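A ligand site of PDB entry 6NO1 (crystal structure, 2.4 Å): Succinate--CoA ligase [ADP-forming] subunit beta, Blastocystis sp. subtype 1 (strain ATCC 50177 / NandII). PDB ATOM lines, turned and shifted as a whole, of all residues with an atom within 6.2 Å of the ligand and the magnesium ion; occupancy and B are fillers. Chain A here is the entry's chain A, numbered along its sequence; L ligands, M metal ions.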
ATOM      1  N   GLU A   5       3.439  10.682 -14.118  1.00  0.00           N
ATOM      2  CA  GLU A   5       2.310  11.266 -13.395  1.00  0.00           C
ATOM      3  C   GLU A   5       2.322  12.783 -13.497  1.00  0.00           C
ATOM      4  O   GLU A   5       1.438  13.377 -14.123  1.00  0.00           O
ATOM      5  CB  GLU A   5       2.350  10.836 -11.930  1.00  0.00           C
ATOM      6  CG  GLU A   5       1.263  11.444 -11.053  1.00  0.00           C
ATOM      7  CD  GLU A   5       1.521  11.223  -9.574  1.00  0.00           C
ATOM      8  OE1 GLU A   5       2.601  10.695  -9.236  1.00  0.00           O
ATOM      9  OE2 GLU A   5       0.650  11.575  -8.759  1.00  0.00           O
ATOM     10  N   LYS A   9      -0.525  15.352 -15.232  1.00  0.00           N
ATOM     11  CA  LYS A   9      -1.315  16.361 -14.531  1.00  0.00           C
ATOM     12  C   LYS A   9      -1.065  17.756 -15.088  1.00  0.00           C
ATOM     13  O   LYS A   9      -1.979  18.577 -15.166  1.00  0.00           O
ATOM     14  CB  LYS A   9      -1.014  16.317 -13.029  1.00  0.00           C
ATOM     15  CG  LYS A   9      -1.482  15.045 -12.343  1.00  0.00           C
ATOM     16  CD  LYS A   9      -1.010  15.011 -10.901  1.00  0.00           C
ATOM     17  CE  LYS A   9      -1.611  13.842 -10.137  1.00  0.00           C
ATOM     18  NZ  LYS A   9      -1.124  13.801  -8.724  1.00  0.00           N
ATOM     19  N   GLN A  20      -3.409  17.825  -8.899  1.00  0.00           N
ATOM     20  CA  GLN A  20      -2.326  18.101  -7.956  1.00  0.00           C
ATOM     21  C   GLN A  20      -1.009  17.617  -8.550  1.00  0.00           C
ATOM     22  O   GLN A  20      -0.511  16.530  -8.239  1.00  0.00           O
ATOM     23  CB  GLN A  20      -2.605  17.444  -6.600  1.00  0.00           C
ATOM     24  CG  GLN A  20      -1.599  17.837  -5.523  1.00  0.00           C
ATOM     25  CD  GLN A  20      -1.863  17.153  -4.188  1.00  0.00           C
ATOM     26  OE1 GLN A  20      -2.161  15.956  -4.144  1.00  0.00           O
ATOM     27  NE2 GLN A  20      -1.741  17.902  -3.110  1.00  0.00           N
ATOM     28  N   VAL A  48       3.223  14.600   0.865  1.00  0.00           N
ATOM     29  CA  VAL A  48       3.131  13.279   0.272  1.00  0.00           C
ATOM     30  C   VAL A  48       4.224  13.154  -0.785  1.00  0.00           C
ATOM     31  O   VAL A  48       4.385  14.037  -1.634  1.00  0.00           O
ATOM     32  CB  VAL A  48       1.748  13.036  -0.363  1.00  0.00           C
ATOM     33  CG1 VAL A  48       1.727  11.709  -1.114  1.00  0.00           C
ATOM     34  CG2 VAL A  48       0.659  13.059   0.703  1.00  0.00           C
ATOM     35  N   LYS A  50       5.676  10.881  -3.842  1.00  0.00           N
ATOM     36  CA  LYS A  50       5.206   9.902  -4.811  1.00  0.00           C
ATOM     37  C   LYS A  50       6.349   9.585  -5.780  1.00  0.00           C
ATOM     38  O   LYS A  50       6.764  10.450  -6.548  1.00  0.00           O
ATOM     39  CB  LYS A  50       3.987  10.420  -5.570  1.00  0.00           C
ATOM     40  CG  LYS A  50       2.933  11.047  -4.673  1.00  0.00           C
ATOM     41  CD  LYS A  50       1.694  11.466  -5.458  1.00  0.00           C
ATOM     42  CE  LYS A  50       0.700  10.329  -5.580  1.00  0.00           C
ATOM     43  NZ  LYS A  50      -0.508  10.715  -6.358  1.00  0.00           N
ATOM     44  N   ALA A  55       4.562   2.670 -13.690  1.00  0.00           N
ATOM     45  CA  ALA A  55       4.002   1.393 -13.244  1.00  0.00           C
ATOM     46  C   ALA A  55       2.982   1.639 -12.148  1.00  0.00           C
ATOM     47  O   ALA A  55       3.143   2.559 -11.328  1.00  0.00           O
ATOM     48  CB  ALA A  55       5.107   0.461 -12.735  1.00  0.00           C
ATOM     49  N   GLY A  56       1.917   0.827 -12.112  1.00  0.00           N
ATOM     50  CA  GLY A  56       0.880   0.985 -11.120  1.00  0.00           C
ATOM     51  C   GLY A  56       1.180   0.226  -9.830  1.00  0.00           C
ATOM     52  O   GLY A  56       2.103  -0.573  -9.752  1.00  0.00           O
ATOM     53  N   GLY A  57       0.362   0.501  -8.816  1.00  0.00           N
ATOM     54  CA  GLY A  57       0.514  -0.162  -7.532  1.00  0.00           C
ATOM     55  C   GLY A  57       1.601   0.413  -6.658  1.00  0.00           C
ATOM     56  O   GLY A  57       2.133  -0.296  -5.804  1.00  0.00           O
ATOM     57  N   ARG A  58       1.940   1.691  -6.839  1.00  0.00           N
ATOM     58  CA  ARG A  58       3.011   2.291  -6.057  1.00  0.00           C
ATOM     59  C   ARG A  58       2.650   2.328  -4.573  1.00  0.00           C
ATOM     60  O   ARG A  58       3.476   1.992  -3.711  1.00  0.00           O
ATOM     61  CB  ARG A  58       3.311   3.698  -6.566  1.00  0.00           C
ATOM     62  CG  ARG A  58       3.708   3.753  -8.038  1.00  0.00           C
ATOM     63  CD  ARG A  58       3.822   5.176  -8.536  1.00  0.00           C
ATOM     64  NE  ARG A  58       2.557   5.902  -8.422  1.00  0.00           N
ATOM     65  CZ  ARG A  58       2.372   7.160  -8.792  1.00  0.00           C
ATOM     66  NH1 ARG A  58       3.379   7.867  -9.305  1.00  0.00           N
ATOM     67  NH2 ARG A  58       1.183   7.730  -8.654  1.00  0.00           N
ATOM     68  N   GLY A  59       1.423   2.747  -4.255  1.00  0.00           N
ATOM     69  CA  GLY A  59       0.992   2.765  -2.868  1.00  0.00           C
ATOM     70  C   GLY A  59       1.022   1.390  -2.239  1.00  0.00           C
ATOM     71  O   GLY A  59       1.177   1.263  -1.016  1.00  0.00           O
ATOM     72  N   LYS A  60       0.872   0.340  -3.050  1.00  0.00           N
ATOM     73  CA  LYS A  60       0.904  -1.025  -2.527  1.00  0.00           C
ATOM     74  C   LYS A  60       2.328  -1.542  -2.351  1.00  0.00           C
ATOM     75  O   LYS A  60       2.592  -2.306  -1.414  1.00  0.00           O
ATOM     76  CB  LYS A  60       0.140  -1.964  -3.470  1.00  0.00           C
ATOM     77  CG  LYS A  60      -1.241  -1.491  -3.865  1.00  0.00           C
ATOM     78  CD  LYS A  60      -2.213  -1.520  -2.701  1.00  0.00           C
ATOM     79  CE  LYS A  60      -3.636  -1.265  -3.168  1.00  0.00           C
ATOM     80  NZ  LYS A  60      -4.624  -1.412  -2.058  1.00  0.00           N
ATOM     81  N   VAL A  71       3.938   5.578  -2.046  1.00  0.00           N
ATOM     82  CA  VAL A  71       3.295   6.864  -1.771  1.00  0.00           C
ATOM     83  C   VAL A  71       3.133   6.982  -0.264  1.00  0.00           C
ATOM     84  O   VAL A  71       2.257   6.339   0.331  1.00  0.00           O
ATOM     85  CB  VAL A  71       1.944   6.979  -2.491  1.00  0.00           C
ATOM     86  CG1 VAL A  71       1.248   8.284  -2.124  1.00  0.00           C
ATOM     87  CG2 VAL A  71       2.132   6.877  -3.999  1.00  0.00           C
ATOM     88  N   LEU A  73       3.207   9.340   3.513  1.00  0.00           N
ATOM     89  CA  LEU A  73       2.934  10.612   4.171  1.00  0.00           C
ATOM     90  C   LEU A  73       4.171  11.098   4.917  1.00  0.00           C
ATOM     91  O   LEU A  73       4.980  10.299   5.414  1.00  0.00           O
ATOM     92  CB  LEU A  73       1.763  10.458   5.136  1.00  0.00           C
ATOM     93  CG  LEU A  73       1.230  11.717   5.813  1.00  0.00           C
ATOM     94  CD1 LEU A  73       0.614  12.660   4.793  1.00  0.00           C
ATOM     95  CD2 LEU A  73       0.211  11.345   6.886  1.00  0.00           C
ATOM     96  N   CYS A 110       3.965  16.648  -3.230  1.00  0.00           N
ATOM     97  CA  CYS A 110       2.722  17.420  -3.195  1.00  0.00           C
ATOM     98  C   CYS A 110       2.215  17.512  -1.766  1.00  0.00           C
ATOM     99  O   CYS A 110       2.556  16.694  -0.906  1.00  0.00           O
ATOM    100  CB  CYS A 110       1.651  16.807  -4.118  1.00  0.00           C
ATOM    101  SG  CYS A 110       1.331  15.051  -3.856  1.00  0.00           S
ATOM    102  N   GLY A 111       1.387  18.515  -1.517  1.00  0.00           N
ATOM    103  CA  GLY A 111       0.849  18.721  -0.188  1.00  0.00           C
ATOM    104  C   GLY A 111      -0.149  17.642   0.185  1.00  0.00           C
ATOM    105  O   GLY A 111      -0.834  17.066  -0.661  1.00  0.00           O
ATOM    106  N   ALA A 112      -0.225  17.366   1.479  1.00  0.00           N
ATOM    107  CA  ALA A 112      -1.168  16.375   1.990  1.00  0.00           C
ATOM    108  C   ALA A 112      -2.554  16.998   2.052  1.00  0.00           C
ATOM    109  O   ALA A 112      -2.762  18.009   2.743  1.00  0.00           O
ATOM    110  CB  ALA A 112      -0.737  15.887   3.365  1.00  0.00           C
ATOM    111  N   VAL A 113      -3.507  16.398   1.339  1.00  0.00           N
ATOM    112  CA  VAL A 113      -4.858  16.924   1.247  1.00  0.00           C
ATOM    113  C   VAL A 113      -5.837  15.904   1.802  1.00  0.00           C
ATOM    114  O   VAL A 113      -5.587  14.698   1.787  1.00  0.00           O
ATOM    115  CB  VAL A 113      -5.223  17.284  -0.204  1.00  0.00           C
ATOM    116  CG1 VAL A 113      -6.651  17.801  -0.288  1.00  0.00           C
ATOM    117  CG2 VAL A 113      -4.244  18.303  -0.759  1.00  0.00           C
ATOM    118  N   LYS A 114      -6.956  16.405   2.321  1.00  0.00           N
ATOM    119  CA  LYS A 114      -8.012  15.541   2.825  1.00  0.00           C
ATOM    120  C   LYS A 114      -8.918  15.120   1.669  1.00  0.00           C
ATOM    121  O   LYS A 114      -9.431  15.970   0.932  1.00  0.00           O
ATOM    122  CB  LYS A 114      -8.823  16.262   3.900  1.00  0.00           C
ATOM    123  CG  LYS A 114      -9.754  15.362   4.678  1.00  0.00           C
ATOM    124  CD  LYS A 114     -10.665  16.148   5.605  1.00  0.00           C
ATOM    125  CE  LYS A 114     -11.567  15.224   6.404  1.00  0.00           C
ATOM    126  NZ  LYS A 114     -12.547  15.981   7.220  1.00  0.00           N
ATOM    127  N   ILE A 115      -9.112  13.812   1.522  1.00  0.00           N
ATOM    128  CA  ILE A 115      -9.874  13.232   0.423  1.00  0.00           C
ATOM    129  C   ILE A 115     -11.219  12.770   0.966  1.00  0.00           C
ATOM    130  O   ILE A 115     -11.264  12.022   1.952  1.00  0.00           O
ATOM    131  CB  ILE A 115      -9.118  12.070  -0.246  1.00  0.00           C
ATOM    132  CG1 ILE A 115      -7.738  12.542  -0.712  1.00  0.00           C
ATOM    133  CG2 ILE A 115      -9.920  11.521  -1.415  1.00  0.00           C
ATOM    134  CD1 ILE A 115      -6.825  11.413  -1.158  1.00  0.00           C
ATOM    135  N   GLU A 118     -13.264   8.997  -3.708  1.00  0.00           N
ATOM    136  CA  GLU A 118     -12.324   8.607  -4.757  1.00  0.00           C
ATOM    137  C   GLU A 118     -13.077   7.845  -5.831  1.00  0.00           C
ATOM    138  O   GLU A 118     -13.827   6.909  -5.529  1.00  0.00           O
ATOM    139  CB  GLU A 118     -11.184   7.747  -4.186  1.00  0.00           C
ATOM    140  CG  GLU A 118     -10.236   8.504  -3.264  1.00  0.00           C
ATOM    141  CD  GLU A 118      -9.040   7.666  -2.844  1.00  0.00           C
ATOM    142  OE1 GLU A 118      -8.961   6.494  -3.260  1.00  0.00           O
ATOM    143  OE2 GLU A 118      -8.175   8.183  -2.107  1.00  0.00           O
ATOM    144  N   GLY A 141      -9.835   3.067  -5.289  1.00  0.00           N
ATOM    145  CA  GLY A 141      -8.788   2.150  -4.900  1.00  0.00           C
ATOM    146  C   GLY A 141      -9.147   0.705  -5.161  1.00  0.00           C
ATOM    147  O   GLY A 141      -9.703   0.033  -4.288  1.00  0.00           O
ATOM    148  N   ASN A 210      -6.913   7.796 -11.862  1.00  0.00           N
ATOM    149  CA  ASN A 210      -7.181   6.839 -10.783  1.00  0.00           C
ATOM    150  C   ASN A 210      -6.299   7.182  -9.597  1.00  0.00           C
ATOM    151  O   ASN A 210      -5.109   6.831  -9.576  1.00  0.00           O
ATOM    152  CB  ASN A 210      -6.943   5.407 -11.246  1.00  0.00           C
ATOM    153  CG  ASN A 210      -7.247   4.389 -10.173  1.00  0.00           C
ATOM    154  OD1 ASN A 210      -6.447   3.490  -9.900  1.00  0.00           O
ATOM    155  ND2 ASN A 210      -8.403   4.522  -9.532  1.00  0.00           N
ATOM    156  N   PRO A 211      -6.848   7.845  -8.554  1.00  0.00           N
ATOM    157  CA  PRO A 211      -8.238   8.263  -8.346  1.00  0.00           C
ATOM    158  C   PRO A 211      -8.557   9.702  -8.773  1.00  0.00           C
ATOM    159  O   PRO A 211      -7.711  10.587  -8.637  1.00  0.00           O
ATOM    160  CB  PRO A 211      -8.402   8.123  -6.841  1.00  0.00           C
ATOM    161  CG  PRO A 211      -7.064   8.508  -6.300  1.00  0.00           C
ATOM    162  CD  PRO A 211      -6.042   8.087  -7.350  1.00  0.00           C
ATOM    163  N   LEU A 227      -5.850  13.220  -8.477  1.00  0.00           N
ATOM    164  CA  LEU A 227      -4.752  12.849  -7.591  1.00  0.00           C
ATOM    165  C   LEU A 227      -3.761  11.912  -8.255  1.00  0.00           C
ATOM    166  O   LEU A 227      -2.784  11.507  -7.613  1.00  0.00           O
ATOM    167  CB  LEU A 227      -5.306  12.205  -6.323  1.00  0.00           C
ATOM    168  CG  LEU A 227      -6.343  13.040  -5.572  1.00  0.00           C
ATOM    169  CD1 LEU A 227      -6.928  12.252  -4.420  1.00  0.00           C
ATOM    170  CD2 LEU A 227      -5.732  14.345  -5.093  1.00  0.00           C
ATOM    171  N   ASP A 228      -3.976  11.549  -9.517  1.00  0.00           N
ATOM    172  CA  ASP A 228      -3.095  10.665 -10.257  1.00  0.00           C
ATOM    173  C   ASP A 228      -3.485  10.750 -11.723  1.00  0.00           C
ATOM    174  O   ASP A 228      -4.630  11.097 -12.049  1.00  0.00           O
ATOM    175  CB  ASP A 228      -3.174   9.220  -9.745  1.00  0.00           C
ATOM    176  CG  ASP A 228      -2.082   8.330 -10.291  1.00  0.00           C
ATOM    177  OD1 ASP A 228      -1.191   8.840 -11.011  1.00  0.00           O
ATOM    178  OD2 ASP A 228      -2.092   7.116  -9.997  1.00  0.00           O
ATOM    179  N   ALA A 229      -2.545  10.435 -12.604  1.00  0.00           N
ATOM    180  CA  ALA A 229      -2.805  10.584 -14.031  1.00  0.00           C
ATOM    181  C   ALA A 229      -1.831   9.732 -14.831  1.00  0.00           C
ATOM    182  O   ALA A 229      -0.640   9.664 -14.525  1.00  0.00           O
ATOM    183  CB  ALA A 229      -2.686  12.050 -14.460  1.00  0.00           C
HETATM  184  P1  LIG L   1      -0.928   4.141  -7.290  1.00  0.00           P
HETATM  185  O1  LIG L   1       0.034   3.807  -8.390  1.00  0.00           O
HETATM  186  O2  LIG L   1      -0.833   3.173  -6.098  1.00  0.00           O
HETATM  187  O3  LIG L   1      -2.392   4.148  -7.766  1.00  0.00           O
HETATM  188  P2  LIG L   1      -1.580   6.858  -6.436  1.00  0.00           P
HETATM  189  O4  LIG L   1      -1.128   8.041  -7.197  1.00  0.00           O
HETATM  190  O5  LIG L   1      -3.025   6.430  -6.712  1.00  0.00           O
HETATM  191  O6  LIG L   1      -0.650   5.591  -6.703  1.00  0.00           O
HETATM  192  O7  LIG L   1      -1.476   7.115  -4.859  1.00  0.00           O
HETATM  193  C1  LIG L   1      -1.851   6.172  -3.835  1.00  0.00           C
HETATM  194  C2  LIG L   1      -2.945   6.777  -2.993  1.00  0.00           C
HETATM  195  O8  LIG L   1      -2.435   7.896  -2.247  1.00  0.00           O
HETATM  196  C3  LIG L   1      -4.122   7.357  -3.769  1.00  0.00           C
HETATM  197  O9  LIG L   1      -5.044   6.347  -4.127  1.00  0.00           O
HETATM  198  C4  LIG L   1      -4.718   8.348  -2.767  1.00  0.00           C
HETATM  199  O10 LIG L   1      -5.676   7.709  -1.916  1.00  0.00           O
HETATM  200  C5  LIG L   1      -3.488   8.782  -1.942  1.00  0.00           C
HETATM  201  N1  LIG L   1      -3.041  10.147  -2.226  1.00  0.00           N
HETATM  202  C6  LIG L   1      -2.516  10.621  -3.391  1.00  0.00           C
HETATM  203  N2  LIG L   1      -2.206  11.895  -3.366  1.00  0.00           N
HETATM  204  C7  LIG L   1      -2.544  12.285  -2.074  1.00  0.00           C
HETATM  205  C8  LIG L   1      -2.465  13.521  -1.400  1.00  0.00           C
HETATM  206  N3  LIG L   1      -1.993  14.641  -1.963  1.00  0.00           N
HETATM  207  N4  LIG L   1      -2.885  13.571  -0.121  1.00  0.00           N
HETATM  208  C9  LIG L   1      -3.358  12.451   0.442  1.00  0.00           C
HETATM  209  N5  LIG L   1      -3.489  11.234  -0.097  1.00  0.00           N
HETATM  210  C10 LIG L   1      -3.062  11.218  -1.363  1.00  0.00           C
HETATM  211 MG    MG M   1      -3.362   5.731  -8.977  1.00  0.00          MG
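The side-chain carboxylate (OE2) of Glu 118 sits at hydrogen-bond distance from an oxygen (O10) of the ligand (2.6 Å). A nitrogen (N3) of the ligand lies within hydrogen-bond range of the side-chain amide oxygen (OE1) of Gln 20, at 2.6 Å. O2 of the ligand sits at hydrogen-bond distance from N of Arg 58, at 3.2 Å. The guanidinium group (NH2) of Arg 58 is in salt-bridge range of an oxygen (O4) of the ligand, 2.7 Å away. NZ of Lys 50 is in salt-bridge range of O4 of the ligand. N of Gly 59 lies within hydrogen-bond range of O2 of the ligand (2.9 Å). A nitrogen (N3) of the ligand lies within hydrogen-bond range of the backbone carbonyl oxygen of Gly 111 (3.0 Å). A nitrogen (N4) of the ligand sits at hydrogen-bond distance from the backbone NH of Val 113 (3.2 Å). N of Gly 57 lies within hydrogen-bond range of O1 of the ligand (3.3 Å).
The side-chain amide nitrogen of Gln 20 lies within hydrogen-bond range of the backbone carbonyl oxygen of Gly 111 (2.7 Å). OE1 of Gln 20 sits at hydrogen-bond distance from SG of Cys 110. The backbone carbonyl oxygen (O) of Gln 20 is in hydrogen-bond range of the side-chain amino group (NZ) of Lys 9 (2.8 Å). NH1 of Arg 58 lies within salt-bridge range of OE1 of Glu 5, at 2.9 Å. NZ of Lys 50 lies within salt-bridge range of OE2 of Glu 5 (2.8 Å). The backbone carbonyl oxygen (O) of Pro 211 is in hydrogen-bond range of the backbone NH (N) of Leu 227 (3.2 Å). The backbone NH (N) of Val 48 is in hydrogen-bond range of the backbone carbonyl oxygen (O) of Cys 110. NZ of Lys 9 is in hydrogen-bond range of O of Leu 227 (3.0 Å).
Val 48 touches the ligand (CG2 to N4, 3.7 Å). CG1 of Val 71 touches O8 of the ligand, 3.7 Å away. Cys 110 touches the ligand (SG to N3, 3.8 Å). Ala 112 touches the ligand (CA to N4, 3.9 Å). Ile 115 touches the ligand. Pro 211 touches the ligand. Leu 227 touches the ligand (O to O4, 3.9 Å). Hydrophobic or aromatic side chains within 4 Å of the ligand: Val 48, Val 71, Ile 115 and Pro 211. Within 4 Å of the ligand: Gln 20, Val 48, Lys 50, Gly 57, Arg 58, Gly 59, Val 71, Cys 110, Gly 111, Ala 112, Val 113, Ile 115, Glu 118, Asn 210, Pro 211, Leu 227 and Asp 228. The nearest printed residue that does not touch the ligand is Gly 56 (4.02 Å).
Merely in contact with the magnesium ion: Pro 211 (3.9 Å).
The magnesium ion is bound by the side-chain carboxylate (OD2) of Asp 228 (2.1 Å), the backbone carbonyl oxygen (O) of Asn 210 (2.1 Å), an oxygen (O3) of the ligand (2.2 Å) and an oxygen (O5) of the ligand (2.4 Å).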
